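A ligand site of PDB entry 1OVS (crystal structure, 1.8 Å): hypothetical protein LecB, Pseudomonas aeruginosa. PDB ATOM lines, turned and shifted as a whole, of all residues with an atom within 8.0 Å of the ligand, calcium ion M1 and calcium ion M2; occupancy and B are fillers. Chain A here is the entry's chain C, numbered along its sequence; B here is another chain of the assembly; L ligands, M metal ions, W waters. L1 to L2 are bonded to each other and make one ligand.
The side-chain carboxylate (OD1) of Asp 101 binds calcium ion M1, 2.3 Å away. Calcium ion M1 is bound by the side-chain carboxylate (OD2) of Asp 104 (2.4 Å). Calcium ion M1 is bound by OE2 of Glu 95 (2.4 Å). Calcium ion M1 is bound by OD1 of Asp 99, at 2.4 Å. Calcium ion M1 is bound by the side-chain carboxylate (OE1) of Glu 95 (2.4 Å). Calcium ion M1 is bound by O2 of LIG L1 (2.6 Å). Calcium ion M1 is bound by the side-chain carboxylate (OD1) of Asp 104. Calcium ion M1 is bound by O3 of LIG L1 (2.7 Å).
Merely in contact with the ligand: Gly 97. Of the 28 residues printed, 10 come within 4 Å of the ligand. The nearest printed residue that does not touch the ligand is Gly 24 (4.3 Å).
Five residues have an atom within 4 Å of calcium ion M2: Asn 21, Asp 101, Asn 103, Asp 104 and Gly 114 of chain B. Along chain A the residues within 4 Å of calcium ion M2 span positions 21 to 104. The nearest printed residue that does not touch calcium ion M2 is Ser 22 (4.5 Å).
Of the 28 residues printed, 4 come within 4 Å of calcium ion M1. Along chain A the residues within 4 Å of calcium ion M1 span positions 95 to 104.
The side-chain amide nitrogen (ND2) of Asn 103 lies within hydrogen-bond range of the backbone carbonyl oxygen (O) of Pro 112 of chain B (2.8 Å). N of Asp 96 lies close to OD2 of Asp 104, 2.8 Å away. The backbone NH of Asp 104 sits at hydrogen-bond distance from the backbone carbonyl oxygen of Ser 94 (3.2 Å). The backbone NH (N) of Gly 97 lies close to the side-chain carboxylate (OE2) of Glu 95, 2.6 Å away. The backbone carbonyl oxygen of Ser 44 is in hydrogen-bond range of the backbone NH of Asn 21, at 3.1 Å. N of Gly 24 sits close to OG of Ser 22 (3.1 Å). The side-chain hydroxyl (OG) of Ser 22 sits at hydrogen-bond distance from the side-chain amide nitrogen (NE2) of Gln 26. The backbone carbonyl oxygen of Ser 22 lies close to the side-chain amide oxygen of Gln 43 (2.9 Å).
Calcium ion M2 is bound by the side-chain amide oxygen (OD1) of Asn 103 (2.3 Å), the side-chain carboxylate (OD2) of Asp 101 (2.4 Å), an oxygen (O2) of LIG L1 (2.4 Å), the backbone carbonyl oxygen (O) of Asn 21 (2.4 Å), the side-chain carboxylate (OD1) of Asp 104 (2.5 Å), the chain-end carboxylate (O) of Gly 114 of chain B (2.5 Å) and an oxygen (O1) of LIG L1 (2.5 Å). Slightly farther from calcium ion M2 lies OD1 of Asp 101 (3.1 Å).
OD1 of Asp 96 lies within hydrogen-bond range of O5 of LIG L1, at 2.7 Å. The side-chain hydroxyl (OG) of Ser 22 sits close to an oxygen (O4) of LIG L1, at 3.5 Å. The backbone NH of Ser 23 sits at hydrogen-bond distance from an oxygen (O4) of LIG L1, 3.1 Å away. The side-chain hydroxyl of Ser 23 lies within hydrogen-bond range of an oxygen (O4) of LIG L1, 3.2 Å away.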
ATOM      1  N   ALA A  20      -5.006  -7.262 -17.327  1.00  0.00           N
ATOM      2  CA  ALA A  20      -5.212  -6.038 -16.560  1.00  0.00           C
ATOM      3  C   ALA A  20      -4.703  -4.824 -17.320  1.00  0.00           C
ATOM      4  O   ALA A  20      -3.651  -4.872 -17.953  1.00  0.00           O
ATOM      5  CB  ALA A  20      -4.529  -6.154 -15.210  1.00  0.00           C
ATOM      6  N   ASN A  21      -5.470  -3.739 -17.256  1.00  0.00           N
ATOM      7  CA  ASN A  21      -5.141  -2.470 -17.909  1.00  0.00           C
ATOM      8  C   ASN A  21      -5.639  -1.368 -16.996  1.00  0.00           C
ATOM      9  O   ASN A  21      -6.596  -0.672 -17.323  1.00  0.00           O
ATOM     10  CB  ASN A  21      -5.859  -2.367 -19.262  1.00  0.00           C
ATOM     11  CG  ASN A  21      -5.277  -3.315 -20.301  1.00  0.00           C
ATOM     12  OD1 ASN A  21      -4.220  -3.048 -20.862  1.00  0.00           O
ATOM     13  ND2 ASN A  21      -5.962  -4.436 -20.528  1.00  0.00           N
ATOM     14  N   SER A  22      -4.980  -1.227 -15.854  1.00  0.00           N
ATOM     15  CA  SER A  22      -5.388  -0.223 -14.868  1.00  0.00           C
ATOM     16  C   SER A  22      -4.299  -0.022 -13.830  1.00  0.00           C
ATOM     17  O   SER A  22      -3.494  -0.914 -13.578  1.00  0.00           O
ATOM     18  CB  SER A  22      -6.680  -0.659 -14.181  1.00  0.00           C
ATOM     19  OG  SER A  22      -7.063   0.239 -13.150  1.00  0.00           O
ATOM     20  N   SER A  23      -4.284   1.164 -13.222  1.00  0.00           N
ATOM     21  CA  SER A  23      -3.315   1.477 -12.196  1.00  0.00           C
ATOM     22  C   SER A  23      -3.714   0.757 -10.913  1.00  0.00           C
ATOM     23  O   SER A  23      -2.884   0.533 -10.033  1.00  0.00           O
ATOM     24  CB  SER A  23      -3.288   2.993 -11.929  1.00  0.00           C
ATOM     25  OG  SER A  23      -4.552   3.429 -11.483  1.00  0.00           O
ATOM     26  N   GLY A  24      -4.979   0.376 -10.819  1.00  0.00           N
ATOM     27  CA  GLY A  24      -5.467  -0.311  -9.640  1.00  0.00           C
ATOM     28  C   GLY A  24      -5.355  -1.823  -9.708  1.00  0.00           C
ATOM     29  O   GLY A  24      -5.476  -2.414 -10.789  1.00  0.00           O
ATOM     30  N   THR A  25      -5.128  -2.453  -8.567  1.00  0.00           N
ATOM     31  CA  THR A  25      -5.010  -3.905  -8.510  1.00  0.00           C
ATOM     32  C   THR A  25      -6.379  -4.516  -8.754  1.00  0.00           C
ATOM     33  O   THR A  25      -7.351  -4.223  -8.044  1.00  0.00           O
ATOM     34  CB  THR A  25      -4.461  -4.358  -7.144  1.00  0.00           C
ATOM     35  OG1 THR A  25      -3.107  -3.897  -6.999  1.00  0.00           O
ATOM     36  CG2 THR A  25      -4.490  -5.882  -7.029  1.00  0.00           C
ATOM     37  N   GLN A  26      -6.448  -5.362  -9.771  1.00  0.00           N
ATOM     38  CA  GLN A  26      -7.695  -6.016 -10.162  1.00  0.00           C
ATOM     39  C   GLN A  26      -7.856  -7.353  -9.462  1.00  0.00           C
ATOM     40  O   GLN A  26      -6.915  -8.127  -9.362  1.00  0.00           O
ATOM     41  CB  GLN A  26      -7.706  -6.237 -11.670  1.00  0.00           C
ATOM     42  CG  GLN A  26      -7.505  -4.983 -12.502  1.00  0.00           C
ATOM     43  CD  GLN A  26      -8.625  -3.985 -12.317  1.00  0.00           C
ATOM     44  OE1 GLN A  26      -9.795  -4.312 -12.525  1.00  0.00           O
ATOM     45  NE2 GLN A  26      -8.280  -2.765 -11.920  1.00  0.00           N
ATOM     46  N   GLN A  43      -1.760  -6.385 -10.983  1.00  0.00           N
ATOM     47  CA  GLN A  43      -1.836  -5.023 -11.473  1.00  0.00           C
ATOM     48  C   GLN A  43      -0.964  -4.881 -12.710  1.00  0.00           C
ATOM     49  O   GLN A  43       0.152  -5.380 -12.753  1.00  0.00           O
ATOM     50  CB  GLN A  43      -1.397  -4.027 -10.405  1.00  0.00           C
ATOM     51  CG  GLN A  43      -1.590  -2.557 -10.825  1.00  0.00           C
ATOM     52  CD  GLN A  43      -0.529  -2.067 -11.799  1.00  0.00           C
ATOM     53  OE1 GLN A  43      -0.796  -1.193 -12.627  1.00  0.00           O
ATOM     54  NE2 GLN A  43       0.679  -2.584 -11.671  1.00  0.00           N
ATOM     55  N   SER A  44      -1.503  -4.192 -13.706  1.00  0.00           N
ATOM     56  CA  SER A  44      -0.797  -3.959 -14.961  1.00  0.00           C
ATOM     57  C   SER A  44      -1.562  -2.953 -15.811  1.00  0.00           C
ATOM     58  O   SER A  44      -2.788  -2.937 -15.813  1.00  0.00           O
ATOM     59  CB  SER A  44      -0.668  -5.269 -15.746  1.00  0.00           C
ATOM     60  OG  SER A  44      -0.070  -5.041 -17.016  1.00  0.00           O
ATOM     61  N   THR A  45      -0.829  -2.099 -16.506  1.00  0.00           N
ATOM     62  CA  THR A  45      -1.434  -1.136 -17.397  1.00  0.00           C
ATOM     63  C   THR A  45      -0.997  -1.501 -18.813  1.00  0.00           C
ATOM     64  O   THR A  45      -1.142  -0.707 -19.736  1.00  0.00           O
ATOM     65  CB  THR A  45      -0.971   0.316 -17.094  1.00  0.00           C
ATOM     66  OG1 THR A  45       0.449   0.355 -16.979  1.00  0.00           O
ATOM     67  CG2 THR A  45      -1.608   0.823 -15.810  1.00  0.00           C
ATOM     68  N   ASN A  46      -0.481  -2.719 -18.977  1.00  0.00           N
ATOM     69  CA  ASN A  46      -0.022  -3.164 -20.288  1.00  0.00           C
ATOM     70  C   ASN A  46      -0.557  -4.535 -20.709  1.00  0.00           C
ATOM     71  O   ASN A  46       0.135  -5.340 -21.323  1.00  0.00           O
ATOM     72  CB  ASN A  46       1.519  -3.157 -20.313  1.00  0.00           C
ATOM     73  CG  ASN A  46       2.072  -3.374 -21.717  1.00  0.00           C
ATOM     74  OD1 ASN A  46       1.614  -2.764 -22.681  1.00  0.00           O
ATOM     75  ND2 ASN A  46       3.083  -4.235 -21.835  1.00  0.00           N
ATOM     76  N   VAL A  69     -12.078  -3.815  -7.364  1.00  0.00           N
ATOM     77  CA  VAL A  69     -10.823  -3.125  -7.133  1.00  0.00           C
ATOM     78  C   VAL A  69     -10.909  -2.569  -5.727  1.00  0.00           C
ATOM     79  O   VAL A  69     -11.782  -1.746  -5.424  1.00  0.00           O
ATOM     80  CB  VAL A  69     -10.636  -1.977  -8.141  1.00  0.00           C
ATOM     81  CG1 VAL A  69      -9.338  -1.229  -7.835  1.00  0.00           C
ATOM     82  CG2 VAL A  69     -10.622  -2.526  -9.560  1.00  0.00           C
ATOM     83  N   SER A  94     -14.401  -4.587 -17.852  1.00  0.00           N
ATOM     84  CA  SER A  94     -14.820  -4.001 -16.584  1.00  0.00           C
ATOM     85  C   SER A  94     -14.270  -2.585 -16.446  1.00  0.00           C
ATOM     86  O   SER A  94     -13.201  -2.287 -16.973  1.00  0.00           O
ATOM     87  CB  SER A  94     -14.358  -4.852 -15.412  1.00  0.00           C
ATOM     88  OG  SER A  94     -12.941  -4.919 -15.334  1.00  0.00           O
ATOM     89  N   GLU A  95     -15.003  -1.741 -15.735  1.00  0.00           N
ATOM     90  CA  GLU A  95     -14.600  -0.365 -15.523  1.00  0.00           C
ATOM     91  C   GLU A  95     -14.551  -0.083 -14.021  1.00  0.00           C
ATOM     92  O   GLU A  95     -15.554  -0.248 -13.322  1.00  0.00           O
ATOM     93  CB  GLU A  95     -15.590   0.588 -16.198  1.00  0.00           C
ATOM     94  CG  GLU A  95     -15.270   2.055 -16.010  1.00  0.00           C
ATOM     95  CD  GLU A  95     -13.845   2.378 -16.421  1.00  0.00           C
ATOM     96  OE1 GLU A  95     -13.485   2.126 -17.593  1.00  0.00           O
ATOM     97  OE2 GLU A  95     -13.078   2.862 -15.557  1.00  0.00           O
ATOM     98  N   ASP A  96     -13.385   0.341 -13.542  1.00  0.00           N
ATOM     99  CA  ASP A  96     -13.221   0.639 -12.125  1.00  0.00           C
ATOM    100  C   ASP A  96     -13.124   2.135 -11.889  1.00  0.00           C
ATOM    101  O   ASP A  96     -12.910   2.583 -10.758  1.00  0.00           O
ATOM    102  CB  ASP A  96     -11.951  -0.022 -11.569  1.00  0.00           C
ATOM    103  CG  ASP A  96     -10.692   0.430 -12.297  1.00  0.00           C
ATOM    104  OD1 ASP A  96     -10.621   1.606 -12.726  1.00  0.00           O
ATOM    105  OD2 ASP A  96      -9.748  -0.385 -12.422  1.00  0.00           O
ATOM    106  N   GLY A  97     -13.288   2.911 -12.962  1.00  0.00           N
ATOM    107  CA  GLY A  97     -13.178   4.351 -12.844  1.00  0.00           C
ATOM    108  C   GLY A  97     -14.216   5.145 -13.599  1.00  0.00           C
ATOM    109  O   GLY A  97     -15.393   4.771 -13.655  1.00  0.00           O
ATOM    110  N   THR A  98     -13.780   6.234 -14.221  1.00  0.00           N
ATOM    111  CA  THR A  98     -14.684   7.108 -14.964  1.00  0.00           C
ATOM    112  C   THR A  98     -14.343   7.299 -16.436  1.00  0.00           C
ATOM    113  O   THR A  98     -15.149   7.881 -17.175  1.00  0.00           O
ATOM    114  CB  THR A  98     -14.719   8.497 -14.308  1.00  0.00           C
ATOM    115  OG1 THR A  98     -13.406   9.051 -14.291  1.00  0.00           O
ATOM    116  CG2 THR A  98     -15.239   8.399 -12.871  1.00  0.00           C
ATOM    117  N   ASP A  99     -13.187   6.818 -16.889  1.00  0.00           N
ATOM    118  CA  ASP A  99     -12.815   7.007 -18.290  1.00  0.00           C
ATOM    119  C   ASP A  99     -13.532   6.057 -19.261  1.00  0.00           C
ATOM    120  O   ASP A  99     -13.445   6.210 -20.474  1.00  0.00           O
ATOM    121  CB  ASP A  99     -11.279   6.902 -18.440  1.00  0.00           C
ATOM    122  CG  ASP A  99     -10.761   5.481 -18.305  1.00  0.00           C
ATOM    123  OD1 ASP A  99     -11.430   4.625 -17.692  1.00  0.00           O
ATOM    124  OD2 ASP A  99      -9.640   5.232 -18.798  1.00  0.00           O
ATOM    125  N   ASN A 100     -14.252   5.106 -18.698  1.00  0.00           N
ATOM    126  CA  ASN A 100     -15.029   4.137 -19.468  1.00  0.00           C
ATOM    127  C   ASN A 100     -14.333   3.420 -20.615  1.00  0.00           C
ATOM    128  O   ASN A 100     -14.894   3.321 -21.708  1.00  0.00           O
ATOM    129  CB  ASN A 100     -16.312   4.782 -20.005  1.00  0.00           C
ATOM    130  CG  ASN A 100     -17.189   5.344 -18.900  1.00  0.00           C
ATOM    131  OD1 ASN A 100     -17.437   4.676 -17.894  1.00  0.00           O
ATOM    132  ND2 ASN A 100     -17.662   6.573 -19.088  1.00  0.00           N
ATOM    133  N   ASP A 101     -13.123   2.932 -20.390  1.00  0.00           N
ATOM    134  CA  ASP A 101     -12.448   2.206 -21.455  1.00  0.00           C
ATOM    135  C   ASP A 101     -12.785   0.722 -21.300  1.00  0.00           C
ATOM    136  O   ASP A 101     -12.550  -0.087 -22.205  1.00  0.00           O
ATOM    137  CB  ASP A 101     -10.928   2.460 -21.450  1.00  0.00           C
ATOM    138  CG  ASP A 101     -10.258   2.107 -20.125  1.00  0.00           C
ATOM    139  OD1 ASP A 101     -10.937   1.709 -19.150  1.00  0.00           O
ATOM    140  OD2 ASP A 101      -9.021   2.247 -20.083  1.00  0.00           O
ATOM    141  N   TYR A 102     -13.375   0.399 -20.153  1.00  0.00           N
ATOM    142  CA  TYR A 102     -13.811  -0.966 -19.845  1.00  0.00           C
ATOM    143  C   TYR A 102     -12.805  -2.086 -20.103  1.00  0.00           C
ATOM    144  O   TYR A 102     -13.184  -3.219 -20.421  1.00  0.00           O
ATOM    145  CB  TYR A 102     -15.127  -1.230 -20.594  1.00  0.00           C
ATOM    146  CG  TYR A 102     -16.323  -0.633 -19.880  1.00  0.00           C
ATOM    147  CD1 TYR A 102     -16.998  -1.351 -18.883  1.00  0.00           C
ATOM    148  CD2 TYR A 102     -16.687   0.702 -20.084  1.00  0.00           C
ATOM    149  CE1 TYR A 102     -18.001  -0.757 -18.124  1.00  0.00           C
ATOM    150  CE2 TYR A 102     -17.690   1.296 -19.325  1.00  0.00           C
ATOM    151  CZ  TYR A 102     -18.335   0.569 -18.345  1.00  0.00           C
ATOM    152  OH  TYR A 102     -19.316   1.160 -17.564  1.00  0.00           O
ATOM    153  N   ASN A 103     -11.532  -1.769 -19.946  1.00  0.00           N
ATOM    154  CA  ASN A 103     -10.469  -2.754 -20.149  1.00  0.00           C
ATOM    155  C   ASN A 103      -9.667  -2.927 -18.878  1.00  0.00           C
ATOM    156  O   ASN A 103      -8.640  -3.597 -18.882  1.00  0.00           O
ATOM    157  CB  ASN A 103      -9.512  -2.291 -21.244  1.00  0.00           C
ATOM    158  CG  ASN A 103      -8.709  -1.069 -20.826  1.00  0.00           C
ATOM    159  OD1 ASN A 103      -8.720  -0.676 -19.655  1.00  0.00           O
ATOM    160  ND2 ASN A 103      -7.973  -0.475 -21.770  1.00  0.00           N
ATOM    161  N   ASP A 104     -10.112  -2.298 -17.788  1.00  0.00           N
ATOM    162  CA  ASP A 104      -9.371  -2.364 -16.534  1.00  0.00           C
ATOM    163  C   ASP A 104      -9.043  -3.787 -16.138  1.00  0.00           C
ATOM    164  O   ASP A 104      -7.951  -4.089 -15.648  1.00  0.00           O
ATOM    165  CB  ASP A 104     -10.135  -1.606 -15.461  1.00  0.00           C
ATOM    166  CG  ASP A 104     -10.351  -0.158 -15.843  1.00  0.00           C
ATOM    167  OD1 ASP A 104      -9.381   0.445 -16.366  1.00  0.00           O
ATOM    168  OD2 ASP A 104     -11.462   0.374 -15.637  1.00  0.00           O
ATOM    169  N   ALA A 105     -10.014  -4.651 -16.371  1.00  0.00           N
ATOM    170  CA  ALA A 105      -9.870  -6.074 -16.151  1.00  0.00           C
ATOM    171  C   ALA A 105     -10.626  -6.641 -17.341  1.00  0.00           C
ATOM    172  O   ALA A 105     -11.812  -6.350 -17.514  1.00  0.00           O
ATOM    173  CB  ALA A 105     -10.525  -6.511 -14.831  1.00  0.00           C
ATOM    174  N   VAL A 106      -9.932  -7.382 -18.180  1.00  0.00           N
ATOM    175  CA  VAL A 106     -10.536  -8.005 -19.355  1.00  0.00           C
ATOM    176  C   VAL A 106     -10.453  -9.507 -19.137  1.00  0.00           C
ATOM    177  O   VAL A 106      -9.375 -10.031 -18.866  1.00  0.00           O
ATOM    178  CB  VAL A 106      -9.770  -7.646 -20.653  1.00  0.00           C
ATOM    179  CG1 VAL A 106     -10.275  -8.499 -21.802  1.00  0.00           C
ATOM    180  CG2 VAL A 106      -9.963  -6.158 -20.975  1.00  0.00           C
ATOM    181  N   PRO B 112      -8.853  -0.964 -26.621  1.00  0.00           N
ATOM    182  CA  PRO B 112      -7.601  -0.287 -26.299  1.00  0.00           C
ATOM    183  C   PRO B 112      -6.966  -0.874 -25.044  1.00  0.00           C
ATOM    184  O   PRO B 112      -7.606  -1.634 -24.314  1.00  0.00           O
ATOM    185  CB  PRO B 112      -8.043   1.154 -26.101  1.00  0.00           C
ATOM    186  CG  PRO B 112      -9.347   0.950 -25.387  1.00  0.00           C
ATOM    187  CD  PRO B 112      -9.991  -0.075 -26.309  1.00  0.00           C
ATOM    188  N   LEU B 113      -5.712  -0.504 -24.805  1.00  0.00           N
ATOM    189  CA  LEU B 113      -4.974  -0.969 -23.639  1.00  0.00           C
ATOM    190  C   LEU B 113      -4.682   0.216 -22.723  1.00  0.00           C
ATOM    191  O   LEU B 113      -4.947   1.357 -23.088  1.00  0.00           O
ATOM    192  CB  LEU B 113      -3.655  -1.595 -24.088  1.00  0.00           C
ATOM    193  CG  LEU B 113      -3.736  -2.728 -25.108  1.00  0.00           C
ATOM    194  CD1 LEU B 113      -2.338  -3.218 -25.435  1.00  0.00           C
ATOM    195  CD2 LEU B 113      -4.599  -3.862 -24.562  1.00  0.00           C
ATOM    196  N   GLY B 114      -4.151  -0.084 -21.552  1.00  0.00           N
ATOM    197  CA  GLY B 114      -3.792   0.944 -20.584  1.00  0.00           C
ATOM    198  C   GLY B 114      -4.863   1.378 -19.600  1.00  0.00           C
ATOM    199  O   GLY B 114      -6.051   1.105 -19.839  1.00  0.00           O
ATOM    200  OXT GLY B 114      -4.491   2.014 -18.591  1.00  0.00           O
HETATM  201  C1  LIG L   1      -5.672   4.008 -15.428  1.00  0.00           C
HETATM  202  C2  LIG L   1      -6.485   3.506 -16.636  1.00  0.00           C
HETATM  203  C3  LIG L   1      -7.988   3.687 -16.362  1.00  0.00           C
HETATM  204  C4  LIG L   1      -8.368   3.005 -15.055  1.00  0.00           C
HETATM  205  C5  LIG L   1      -7.522   3.604 -13.942  1.00  0.00           C
HETATM  206  C6  LIG L   1      -7.810   3.050 -12.563  1.00  0.00           C
HETATM  207  O1  LIG L   1      -6.203   2.142 -16.890  1.00  0.00           O
HETATM  208  O2  LIG L   1      -8.735   3.140 -17.428  1.00  0.00           O
HETATM  209  O3  LIG L   1      -9.746   3.207 -14.773  1.00  0.00           O
HETATM  210  O4  LIG L   1      -6.124   3.387 -14.224  1.00  0.00           O
HETATM  211  O5  LIG L   1      -8.985   3.637 -12.028  1.00  0.00           O
HETATM  212  O1  LG2 L   2      -5.751   5.409 -15.356  1.00  0.00           O
HETATM  213 CA    CA M   1     -11.169   2.373 -16.914  1.00  0.00          CA
HETATM  214 CA    CA M   2      -8.011   1.053 -18.307  1.00  0.00          CA
HETATM  215  O   HOH W   1     -10.993   5.901 -15.067  1.00  0.00           O
HETATM  216  O   HOH W   2     -10.375   5.339 -10.215  1.00  0.00           O
